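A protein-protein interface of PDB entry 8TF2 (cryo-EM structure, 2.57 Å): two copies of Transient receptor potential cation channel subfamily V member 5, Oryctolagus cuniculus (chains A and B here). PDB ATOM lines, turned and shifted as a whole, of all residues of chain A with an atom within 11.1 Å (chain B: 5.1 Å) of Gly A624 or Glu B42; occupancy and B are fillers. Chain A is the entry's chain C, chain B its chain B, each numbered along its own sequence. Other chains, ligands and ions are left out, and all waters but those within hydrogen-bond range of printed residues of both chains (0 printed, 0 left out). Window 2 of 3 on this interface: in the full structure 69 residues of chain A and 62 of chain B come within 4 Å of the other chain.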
ATOM      1  N   HIS A 265      -5.269   8.852 -13.885  1.00  0.00           N
ATOM      2  CA  HIS A 265      -4.666   9.977 -13.178  1.00  0.00           C
ATOM      3  C   HIS A 265      -3.184   9.697 -12.947  1.00  0.00           C
ATOM      4  O   HIS A 265      -2.834   8.667 -12.380  1.00  0.00           O
ATOM      5  CB  HIS A 265      -5.433  10.172 -11.867  1.00  0.00           C
ATOM      6  CG  HIS A 265      -4.859  11.243 -10.990  1.00  0.00           C
ATOM      7  ND1 HIS A 265      -4.064  11.031  -9.864  1.00  0.00           N
ATOM      8  CD2 HIS A 265      -5.001  12.583 -11.187  1.00  0.00           C
ATOM      9  CE1 HIS A 265      -3.754  12.250  -9.401  1.00  0.00           C
ATOM     10  NE2 HIS A 265      -4.302  13.199 -10.177  1.00  0.00           N
ATOM     11  N   GLN A 267      -0.250  10.054 -10.744  1.00  0.00           N
ATOM     12  CA  GLN A 267       0.019  10.415  -9.353  1.00  0.00           C
ATOM     13  C   GLN A 267       1.324  11.192  -9.222  1.00  0.00           C
ATOM     14  O   GLN A 267       1.366  12.225  -8.562  1.00  0.00           O
ATOM     15  CB  GLN A 267       0.099   9.159  -8.483  1.00  0.00           C
ATOM     16  CG  GLN A 267      -1.236   8.429  -8.335  1.00  0.00           C
ATOM     17  CD  GLN A 267      -1.079   7.188  -7.482  1.00  0.00           C
ATOM     18  OE1 GLN A 267      -0.149   6.417  -7.657  1.00  0.00           O
ATOM     19  NE2 GLN A 267      -1.962   6.942  -6.547  1.00  0.00           N
ATOM     20  N   TRP A 268       2.390  10.695  -9.841  1.00  0.00           N
ATOM     21  CA  TRP A 268       3.710  11.309  -9.863  1.00  0.00           C
ATOM     22  C   TRP A 268       4.546  10.744 -11.007  1.00  0.00           C
ATOM     23  O   TRP A 268       4.320   9.627 -11.466  1.00  0.00           O
ATOM     24  CB  TRP A 268       4.417  11.094  -8.512  1.00  0.00           C
ATOM     25  CG  TRP A 268       4.573   9.683  -8.035  1.00  0.00           C
ATOM     26  CD1 TRP A 268       3.785   9.077  -7.122  1.00  0.00           C
ATOM     27  CD2 TRP A 268       5.567   8.684  -8.418  1.00  0.00           C
ATOM     28  NE1 TRP A 268       4.227   7.793  -6.907  1.00  0.00           N
ATOM     29  CE2 TRP A 268       5.316   7.492  -7.684  1.00  0.00           C
ATOM     30  CE3 TRP A 268       6.663   8.659  -9.300  1.00  0.00           C
ATOM     31  CZ2 TRP A 268       6.087   6.334  -7.833  1.00  0.00           C
ATOM     32  CZ3 TRP A 268       7.444   7.505  -9.466  1.00  0.00           C
ATOM     33  CH2 TRP A 268       7.156   6.340  -8.740  1.00  0.00           C
ATOM     34  N   LEU A 277      -2.864   5.942 -11.712  1.00  0.00           N
ATOM     35  CA  LEU A 277      -4.022   5.340 -11.087  1.00  0.00           C
ATOM     36  C   LEU A 277      -5.143   5.266 -12.129  1.00  0.00           C
ATOM     37  O   LEU A 277      -5.544   6.286 -12.672  1.00  0.00           O
ATOM     38  CB  LEU A 277      -4.335   6.209  -9.860  1.00  0.00           C
ATOM     39  CG  LEU A 277      -5.330   5.592  -8.885  1.00  0.00           C
ATOM     40  CD1 LEU A 277      -4.706   4.415  -8.135  1.00  0.00           C
ATOM     41  CD2 LEU A 277      -5.775   6.639  -7.882  1.00  0.00           C
ATOM     42  N   ILE A 618      -7.976  -1.104  -5.628  1.00  0.00           N
ATOM     43  CA  ILE A 618      -7.771  -0.204  -4.500  1.00  0.00           C
ATOM     44  C   ILE A 618      -9.074   0.544  -4.232  1.00  0.00           C
ATOM     45  O   ILE A 618      -9.554   1.253  -5.109  1.00  0.00           O
ATOM     46  CB  ILE A 618      -6.639   0.780  -4.868  1.00  0.00           C
ATOM     47  CG1 ILE A 618      -5.304   0.073  -5.180  1.00  0.00           C
ATOM     48  CG2 ILE A 618      -6.430   1.823  -3.771  1.00  0.00           C
ATOM     49  CD1 ILE A 618      -4.274   0.981  -5.836  1.00  0.00           C
ATOM     50  N   CYS A 619      -9.631   0.433  -3.033  1.00  0.00           N
ATOM     51  CA  CYS A 619     -10.835   1.161  -2.653  1.00  0.00           C
ATOM     52  C   CYS A 619     -10.541   2.649  -2.451  1.00  0.00           C
ATOM     53  O   CYS A 619      -9.796   3.029  -1.553  1.00  0.00           O
ATOM     54  CB  CYS A 619     -11.400   0.526  -1.384  1.00  0.00           C
ATOM     55  SG  CYS A 619     -13.002   1.268  -1.005  1.00  0.00           S
ATOM     56  N   GLY A 620     -11.152   3.519  -3.253  1.00  0.00           N
ATOM     57  CA  GLY A 620     -10.971   4.962  -3.158  1.00  0.00           C
ATOM     58  C   GLY A 620     -11.510   5.592  -1.877  1.00  0.00           C
ATOM     59  O   GLY A 620     -10.988   6.613  -1.435  1.00  0.00           O
ATOM     60  N   TYR A 621     -12.503   4.977  -1.235  1.00  0.00           N
ATOM     61  CA  TYR A 621     -13.103   5.495  -0.006  1.00  0.00           C
ATOM     62  C   TYR A 621     -12.104   5.543   1.159  1.00  0.00           C
ATOM     63  O   TYR A 621     -12.171   6.435   2.002  1.00  0.00           O
ATOM     64  CB  TYR A 621     -14.330   4.651   0.354  1.00  0.00           C
ATOM     65  CG  TYR A 621     -15.086   5.182   1.555  1.00  0.00           C
ATOM     66  CD1 TYR A 621     -16.010   6.229   1.388  1.00  0.00           C
ATOM     67  CD2 TYR A 621     -14.823   4.670   2.836  1.00  0.00           C
ATOM     68  CE1 TYR A 621     -16.661   6.778   2.511  1.00  0.00           C
ATOM     69  CE2 TYR A 621     -15.465   5.224   3.964  1.00  0.00           C
ATOM     70  CZ  TYR A 621     -16.377   6.283   3.801  1.00  0.00           C
ATOM     71  OH  TYR A 621     -16.984   6.823   4.892  1.00  0.00           O
ATOM     72  N   GLU A 622     -11.119   4.643   1.180  1.00  0.00           N
ATOM     73  CA  GLU A 622     -10.048   4.645   2.181  1.00  0.00           C
ATOM     74  C   GLU A 622      -9.119   5.868   2.088  1.00  0.00           C
ATOM     75  O   GLU A 622      -8.398   6.145   3.043  1.00  0.00           O
ATOM     76  CB  GLU A 622      -9.220   3.358   2.072  1.00  0.00           C
ATOM     77  CG  GLU A 622     -10.063   2.097   2.301  1.00  0.00           C
ATOM     78  CD  GLU A 622      -9.224   0.817   2.455  1.00  0.00           C
ATOM     79  OE1 GLU A 622      -8.075   0.874   2.952  1.00  0.00           O
ATOM     80  OE2 GLU A 622      -9.731  -0.274   2.123  1.00  0.00           O
ATOM     81  N   TYR A 623      -9.145   6.604   0.967  1.00  0.00           N
ATOM     82  CA  TYR A 623      -8.210   7.684   0.638  1.00  0.00           C
ATOM     83  C   TYR A 623      -8.886   9.002   0.242  1.00  0.00           C
ATOM     84  O   TYR A 623      -8.246   9.880  -0.340  1.00  0.00           O
ATOM     85  CB  TYR A 623      -7.242   7.215  -0.452  1.00  0.00           C
ATOM     86  CG  TYR A 623      -6.614   5.872  -0.175  1.00  0.00           C
ATOM     87  CD1 TYR A 623      -5.633   5.746   0.825  1.00  0.00           C
ATOM     88  CD2 TYR A 623      -7.056   4.742  -0.879  1.00  0.00           C
ATOM     89  CE1 TYR A 623      -5.080   4.484   1.104  1.00  0.00           C
ATOM     90  CE2 TYR A 623      -6.510   3.483  -0.596  1.00  0.00           C
ATOM     91  CZ  TYR A 623      -5.512   3.355   0.386  1.00  0.00           C
ATOM     92  OH  TYR A 623      -4.948   2.150   0.617  1.00  0.00           O
ATOM     93  N   GLY A 624     -10.188   9.140   0.493  1.00  0.00           N
ATOM     94  CA  GLY A 624     -10.967  10.337   0.160  1.00  0.00           C
ATOM     95  C   GLY A 624     -11.306  10.508  -1.324  1.00  0.00           C
ATOM     96  O   GLY A 624     -11.712  11.595  -1.728  1.00  0.00           O
ATOM     97  N   LEU A 625     -11.149   9.460  -2.141  1.00  0.00           N
ATOM     98  CA  LEU A 625     -11.420   9.460  -3.585  1.00  0.00           C
ATOM     99  C   LEU A 625     -12.866   9.074  -3.959  1.00  0.00           C
ATOM    100  O   LEU A 625     -13.177   8.930  -5.141  1.00  0.00           O
ATOM    101  CB  LEU A 625     -10.406   8.540  -4.283  1.00  0.00           C
ATOM    102  CG  LEU A 625      -8.945   8.992  -4.190  1.00  0.00           C
ATOM    103  CD1 LEU A 625      -8.046   7.873  -4.699  1.00  0.00           C
ATOM    104  CD2 LEU A 625      -8.697  10.237  -5.030  1.00  0.00           C
ATOM    105  N   GLY A 626     -13.687   8.782  -2.968  1.00  0.00           N
ATOM    106  CA  GLY A 626     -15.076   8.454  -3.295  1.00  0.00           C
ATOM    107  C   GLY A 626     -15.340   6.973  -3.297  1.00  0.00           C
ATOM    108  O   GLY A 626     -14.611   6.249  -2.628  1.00  0.00           O
ATOM    109  N   ASP A 627     -16.363   6.547  -4.025  1.00  0.00           N
ATOM    110  CA  ASP A 627     -16.779   5.126  -4.031  1.00  0.00           C
ATOM    111  C   ASP A 627     -16.117   4.387  -5.178  1.00  0.00           C
ATOM    112  O   ASP A 627     -16.530   3.264  -5.449  1.00  0.00           O
ATOM    113  CB  ASP A 627     -18.289   5.016  -4.196  1.00  0.00           C
ATOM    114  CG  ASP A 627     -19.037   5.152  -2.880  1.00  0.00           C
ATOM    115  OD1 ASP A 627     -18.391   5.004  -1.817  1.00  0.00           O
ATOM    116  OD2 ASP A 627     -20.259   5.404  -2.927  1.00  0.00           O
ATOM    117  N   ARG A 628     -15.150   5.007  -5.833  1.00  0.00           N
ATOM    118  CA  ARG A 628     -14.564   4.329  -7.000  1.00  0.00           C
ATOM    119  C   ARG A 628     -13.426   3.418  -6.576  1.00  0.00           C
ATOM    120  O   ARG A 628     -12.831   3.638  -5.532  1.00  0.00           O
ATOM    121  CB  ARG A 628     -14.046   5.317  -8.047  1.00  0.00           C
ATOM    122  CG  ARG A 628     -15.112   6.175  -8.708  1.00  0.00           C
ATOM    123  CD  ARG A 628     -14.477   7.099  -9.728  1.00  0.00           C
ATOM    124  NE  ARG A 628     -13.612   8.097  -9.111  1.00  0.00           N
ATOM    125  CZ  ARG A 628     -12.712   8.817  -9.767  1.00  0.00           C
ATOM    126  NH1 ARG A 628     -11.970   9.699  -9.119  1.00  0.00           N
ATOM    127  NH2 ARG A 628     -12.544   8.643 -11.065  1.00  0.00           N
ATOM    128  N   TRP A 629     -13.182   2.404  -7.373  1.00  0.00           N
ATOM    129  CA  TRP A 629     -12.059   1.485  -7.184  1.00  0.00           C
ATOM    130  C   TRP A 629     -11.047   1.650  -8.310  1.00  0.00           C
ATOM    131  O   TRP A 629     -11.411   1.962  -9.439  1.00  0.00           O
ATOM    132  CB  TRP A 629     -12.547   0.041  -7.071  1.00  0.00           C
ATOM    133  CG  TRP A 629     -13.173  -0.325  -5.762  1.00  0.00           C
ATOM    134  CD1 TRP A 629     -14.313   0.187  -5.253  1.00  0.00           C
ATOM    135  CD2 TRP A 629     -12.692  -1.274  -4.765  1.00  0.00           C
ATOM    136  NE1 TRP A 629     -14.569  -0.371  -4.021  1.00  0.00           N
ATOM    137  CE2 TRP A 629     -13.607  -1.288  -3.672  1.00  0.00           C
ATOM    138  CE3 TRP A 629     -11.581  -2.128  -4.673  1.00  0.00           C
ATOM    139  CZ2 TRP A 629     -13.441  -2.119  -2.562  1.00  0.00           C
ATOM    140  CZ3 TRP A 629     -11.391  -2.960  -3.555  1.00  0.00           C
ATOM    141  CH2 TRP A 629     -12.316  -2.957  -2.502  1.00  0.00           C
ATOM    142  N   PHE A 630      -9.773   1.441  -8.008  1.00  0.00           N
ATOM    143  CA  PHE A 630      -8.677   1.773  -8.910  1.00  0.00           C
ATOM    144  C   PHE A 630      -7.651   0.663  -9.050  1.00  0.00           C
ATOM    145  O   PHE A 630      -7.489  -0.161  -8.164  1.00  0.00           O
ATOM    146  CB  PHE A 630      -7.959   3.030  -8.418  1.00  0.00           C
ATOM    147  CG  PHE A 630      -8.831   4.249  -8.262  1.00  0.00           C
ATOM    148  CD1 PHE A 630      -9.069   5.084  -9.367  1.00  0.00           C
ATOM    149  CD2 PHE A 630      -9.407   4.548  -7.018  1.00  0.00           C
ATOM    150  CE1 PHE A 630      -9.890   6.209  -9.229  1.00  0.00           C
ATOM    151  CE2 PHE A 630     -10.232   5.671  -6.886  1.00  0.00           C
ATOM    152  CZ  PHE A 630     -10.471   6.501  -7.987  1.00  0.00           C
ATOM    153  N   ARG A 632      -3.446   0.758  -9.526  1.00  0.00           N
ATOM    154  CA  ARG A 632      -2.237   1.600  -9.652  1.00  0.00           C
ATOM    155  C   ARG A 632      -1.208   0.851 -10.473  1.00  0.00           C
ATOM    156  O   ARG A 632      -0.867  -0.267 -10.117  1.00  0.00           O
ATOM    157  CB  ARG A 632      -1.627   2.017  -8.308  1.00  0.00           C
ATOM    158  CG  ARG A 632      -0.485   3.012  -8.429  1.00  0.00           C
ATOM    159  CD  ARG A 632       0.267   3.151  -7.125  1.00  0.00           C
ATOM    160  NE  ARG A 632       1.146   2.017  -6.905  1.00  0.00           N
ATOM    161  CZ  ARG A 632       2.441   2.002  -7.168  1.00  0.00           C
ATOM    162  NH1 ARG A 632       3.145   0.910  -6.940  1.00  0.00           N
ATOM    163  NH2 ARG A 632       3.035   3.075  -7.649  1.00  0.00           N
ATOM    164  N   MET B  38      -0.900   5.385  -2.245  1.00  0.00           N
ATOM    165  CA  MET B  38      -2.206   5.983  -1.968  1.00  0.00           C
ATOM    166  C   MET B  38      -2.184   6.890  -0.735  1.00  0.00           C
ATOM    167  O   MET B  38      -2.666   8.018  -0.795  1.00  0.00           O
ATOM    168  CB  MET B  38      -3.262   4.900  -1.768  1.00  0.00           C
ATOM    169  CG  MET B  38      -3.483   3.986  -2.965  1.00  0.00           C
ATOM    170  SD  MET B  38      -3.806   4.796  -4.539  1.00  0.00           S
ATOM    171  CE  MET B  38      -5.401   5.565  -4.190  1.00  0.00           C
ATOM    172  N   LEU B  39      -1.581   6.436   0.366  1.00  0.00           N
ATOM    173  CA  LEU B  39      -1.436   7.217   1.594  1.00  0.00           C
ATOM    174  C   LEU B  39      -0.603   8.475   1.367  1.00  0.00           C
ATOM    175  O   LEU B  39      -0.973   9.546   1.839  1.00  0.00           O
ATOM    176  CB  LEU B  39      -0.781   6.360   2.685  1.00  0.00           C
ATOM    177  CG  LEU B  39      -1.640   5.203   3.205  1.00  0.00           C
ATOM    178  CD1 LEU B  39      -0.768   4.266   4.033  1.00  0.00           C
ATOM    179  CD2 LEU B  39      -2.782   5.698   4.083  1.00  0.00           C
ATOM    180  N   GLN B  40       0.491   8.373   0.610  1.00  0.00           N
ATOM    181  CA  GLN B  40       1.319   9.513   0.228  1.00  0.00           C
ATOM    182  C   GLN B  40       0.505  10.591  -0.494  1.00  0.00           C
ATOM    183  O   GLN B  40       0.545  11.755  -0.107  1.00  0.00           O
ATOM    184  CB  GLN B  40       2.498   9.001  -0.607  1.00  0.00           C
ATOM    185  CG  GLN B  40       3.329  10.138  -1.208  1.00  0.00           C
ATOM    186  CD  GLN B  40       4.743   9.691  -1.550  1.00  0.00           C
ATOM    187  OE1 GLN B  40       4.965   8.827  -2.383  1.00  0.00           O
ATOM    188  NE2 GLN B  40       5.742  10.265  -0.932  1.00  0.00           N
ATOM    189  N   GLN B  41      -0.288  10.216  -1.497  1.00  0.00           N
ATOM    190  CA  GLN B  41      -1.126  11.174  -2.217  1.00  0.00           C
ATOM    191  C   GLN B  41      -2.234  11.759  -1.340  1.00  0.00           C
ATOM    192  O   GLN B  41      -2.472  12.961  -1.386  1.00  0.00           O
ATOM    193  CB  GLN B  41      -1.685  10.520  -3.489  1.00  0.00           C
ATOM    194  CG  GLN B  41      -0.590  10.196  -4.519  1.00  0.00           C
ATOM    195  CD  GLN B  41       0.219  11.420  -4.924  1.00  0.00           C
ATOM    196  OE1 GLN B  41      -0.312  12.446  -5.322  1.00  0.00           O
ATOM    197  NE2 GLN B  41       1.525  11.371  -4.834  1.00  0.00           N
ATOM    198  N   GLU B  42      -2.866  10.961  -0.481  1.00  0.00           N
ATOM    199  CA  GLU B  42      -3.865  11.453   0.469  1.00  0.00           C
ATOM    200  C   GLU B  42      -3.272  12.460   1.460  1.00  0.00           C
ATOM    201  O   GLU B  42      -3.820  13.540   1.640  1.00  0.00           O
ATOM    202  CB  GLU B  42      -4.497  10.269   1.207  1.00  0.00           C
ATOM    203  CG  GLU B  42      -5.633  10.736   2.117  1.00  0.00           C
ATOM    204  CD  GLU B  42      -6.214   9.612   2.979  1.00  0.00           C
ATOM    205  OE1 GLU B  42      -5.453   8.729   3.425  1.00  0.00           O
ATOM    206  OE2 GLU B  42      -7.432   9.645   3.263  1.00  0.00           O
ATOM    207  N   ARG B  43      -2.126  12.153   2.074  1.00  0.00           N
ATOM    208  CA  ARG B  43      -1.465  13.053   3.029  1.00  0.00           C
ATOM    209  C   ARG B  43      -1.010  14.358   2.385  1.00  0.00           C
ATOM    210  O   ARG B  43      -1.002  15.377   3.066  1.00  0.00           O
ATOM    211  CB  ARG B  43      -0.297  12.322   3.706  1.00  0.00           C
ATOM    212  CG  ARG B  43      -0.786  11.320   4.765  1.00  0.00           C
ATOM    213  CD  ARG B  43      -1.175  11.991   6.090  1.00  0.00           C
ATOM    214  NE  ARG B  43       0.013  12.469   6.824  1.00  0.00           N
ATOM    215  CZ  ARG B  43       0.776  11.764   7.639  1.00  0.00           C
ATOM    216  NH1 ARG B  43       1.820  12.306   8.186  1.00  0.00           N
ATOM    217  NH2 ARG B  43       0.537  10.517   7.916  1.00  0.00           N
ATOM    218  N   ILE B  44      -0.688  14.355   1.092  1.00  0.00           N
ATOM    219  CA  ILE B  44      -0.486  15.584   0.323  1.00  0.00           C
ATOM    220  C   ILE B  44      -1.811  16.348   0.189  1.00  0.00           C
ATOM    221  O   ILE B  44      -1.850  17.505   0.579  1.00  0.00           O
ATOM    222  CB  ILE B  44       0.197  15.301  -1.032  1.00  0.00           C
ATOM    223  CG1 ILE B  44       1.643  14.805  -0.823  1.00  0.00           C
ATOM    224  CG2 ILE B  44       0.208  16.563  -1.911  1.00  0.00           C
ATOM    225  CD1 ILE B  44       2.252  14.124  -2.055  1.00  0.00           C
ATOM    226  N   ARG B  45      -2.905  15.724  -0.278  1.00  0.00           N
ATOM    227  CA  ARG B  45      -4.228  16.375  -0.401  1.00  0.00           C
ATOM    228  C   ARG B  45      -4.729  16.971   0.916  1.00  0.00           C
ATOM    229  O   ARG B  45      -5.282  18.067   0.929  1.00  0.00           O
ATOM    230  CB  ARG B  45      -5.288  15.392  -0.919  1.00  0.00           C
ATOM    231  CG  ARG B  45      -5.148  15.039  -2.399  1.00  0.00           C
ATOM    232  CD  ARG B  45      -6.382  14.283  -2.907  1.00  0.00           C
ATOM    233  NE  ARG B  45      -6.530  12.936  -2.317  1.00  0.00           N
ATOM    234  CZ  ARG B  45      -6.004  11.818  -2.769  1.00  0.00           C
ATOM    235  NH1 ARG B  45      -6.238  10.684  -2.181  1.00  0.00           N
ATOM    236  NH2 ARG B  45      -5.229  11.799  -3.807  1.00  0.00           N
ATOM    237  N   ASP B  46      -4.534  16.259   2.016  1.00  0.00           N
ATOM    238  CA  ASP B  46      -4.999  16.629   3.353  1.00  0.00           C
ATOM    239  C   ASP B  46      -4.140  17.696   4.058  1.00  0.00           C
ATOM    240  O   ASP B  46      -4.556  18.213   5.094  1.00  0.00           O
ATOM    241  CB  ASP B  46      -5.088  15.363   4.220  1.00  0.00           C
ATOM    242  CG  ASP B  46      -6.180  14.360   3.808  1.00  0.00           C
ATOM    243  OD1 ASP B  46      -6.984  14.639   2.890  1.00  0.00           O
ATOM    244  OD2 ASP B  46      -6.296  13.316   4.489  1.00  0.00           O
ATOM    245  N   SER B  47      -2.956  18.039   3.540  1.00  0.00           N
ATOM    246  CA  SER B  47      -2.036  18.998   4.177  1.00  0.00           C
ATOM    247  C   SER B  47      -1.807  20.204   3.259  1.00  0.00           C
ATOM    248  O   SER B  47      -1.172  20.044   2.219  1.00  0.00           O
ATOM    249  CB  SER B  47      -0.695  18.324   4.489  1.00  0.00           C
ATOM    250  OG  SER B  47      -0.863  17.097   5.169  1.00  0.00           O
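OE1 of Gln B41 touches O of Gln A267 (3.7 Å). Leu A277 touches Met B38 (CD1 to SD, 3.7 Å). Met B38 touches Ile A618. Glu B42 touches Glu A622 (OE2 to O, 3.6 Å). Tyr A623 touches Met B38. Leu B39 touches Tyr A623 (CD2 to CE1, 3.95 Å). Glu B42 touches Tyr A623 (OE2 to CA, 3.4 Å). Glu B42 touches Gly A624 (OE2 to N, 3.9 Å). Met B38 touches Leu A625. Arg B45 touches Leu A625.
Of the 10 printed residues of chain B, 5 touch a printed residue of chain A. Hydrophobic or aromatic side chains of chain B that line the printed part of chain A: Met B38 and Leu B39. Along chain B the printed residues that touch a printed residue of chain A span positions 38 to 45. Among the printed residues, no Asp or Glu carboxylate lies within 4 Å of a Lys or Arg side-chain nitrogen of the other chain.
NH1 of Arg B45 is in hydrogen-bond range of O of Tyr A623 (2.8 Å). SD of Met B38 lies within hydrogen-bond range of NE2 of Gln A267.
No position is printed for both chains.
Of chain B, only Glu B42 (3.9 Å) comes within 4 Å of Gly A624. Of chain A, only Glu A622 (3.6 Å), Tyr A623 (3.4 Å) and Gly A624 (3.9 Å) come within 4 Å of Glu B42. Of chain A, only Tyr A623 (3.95 Å) comes within 4 Å of Leu B39. Arg B45 touches just these residues of chain A: Tyr A623 (2.8 Å) and Leu A625 (3.8 Å). No residue of chain A comes within 4 Å of Asp B46. Of the printed residues of chain B, Leu A625 touches Met B38 (3.5 Å) and Arg B45 (3.8 Å). Printed residues of chain B within 4 Å of Glu A622: Glu B42. Printed residues of chain B within 4 Å of Ile A618: Met B38 (3.7 Å). The nearest residue of chain A that does not touch Glu B42 is Tyr A621 (5.9 Å). The nearest printed residue of chain B that does not touch Gln A267 is Arg B45 (6.5 Å).
N of Leu A625 sits at hydrogen-bond distance from O of Gly A620 (2.9 Å). The backbone NH of Ile A618 is in hydrogen-bond range of the backbone carbonyl oxygen of Phe A630, 2.7 Å away. The backbone NH (N) of Leu A277 is in hydrogen-bond range of the backbone carbonyl oxygen (O) of His A265 (2.8 Å).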
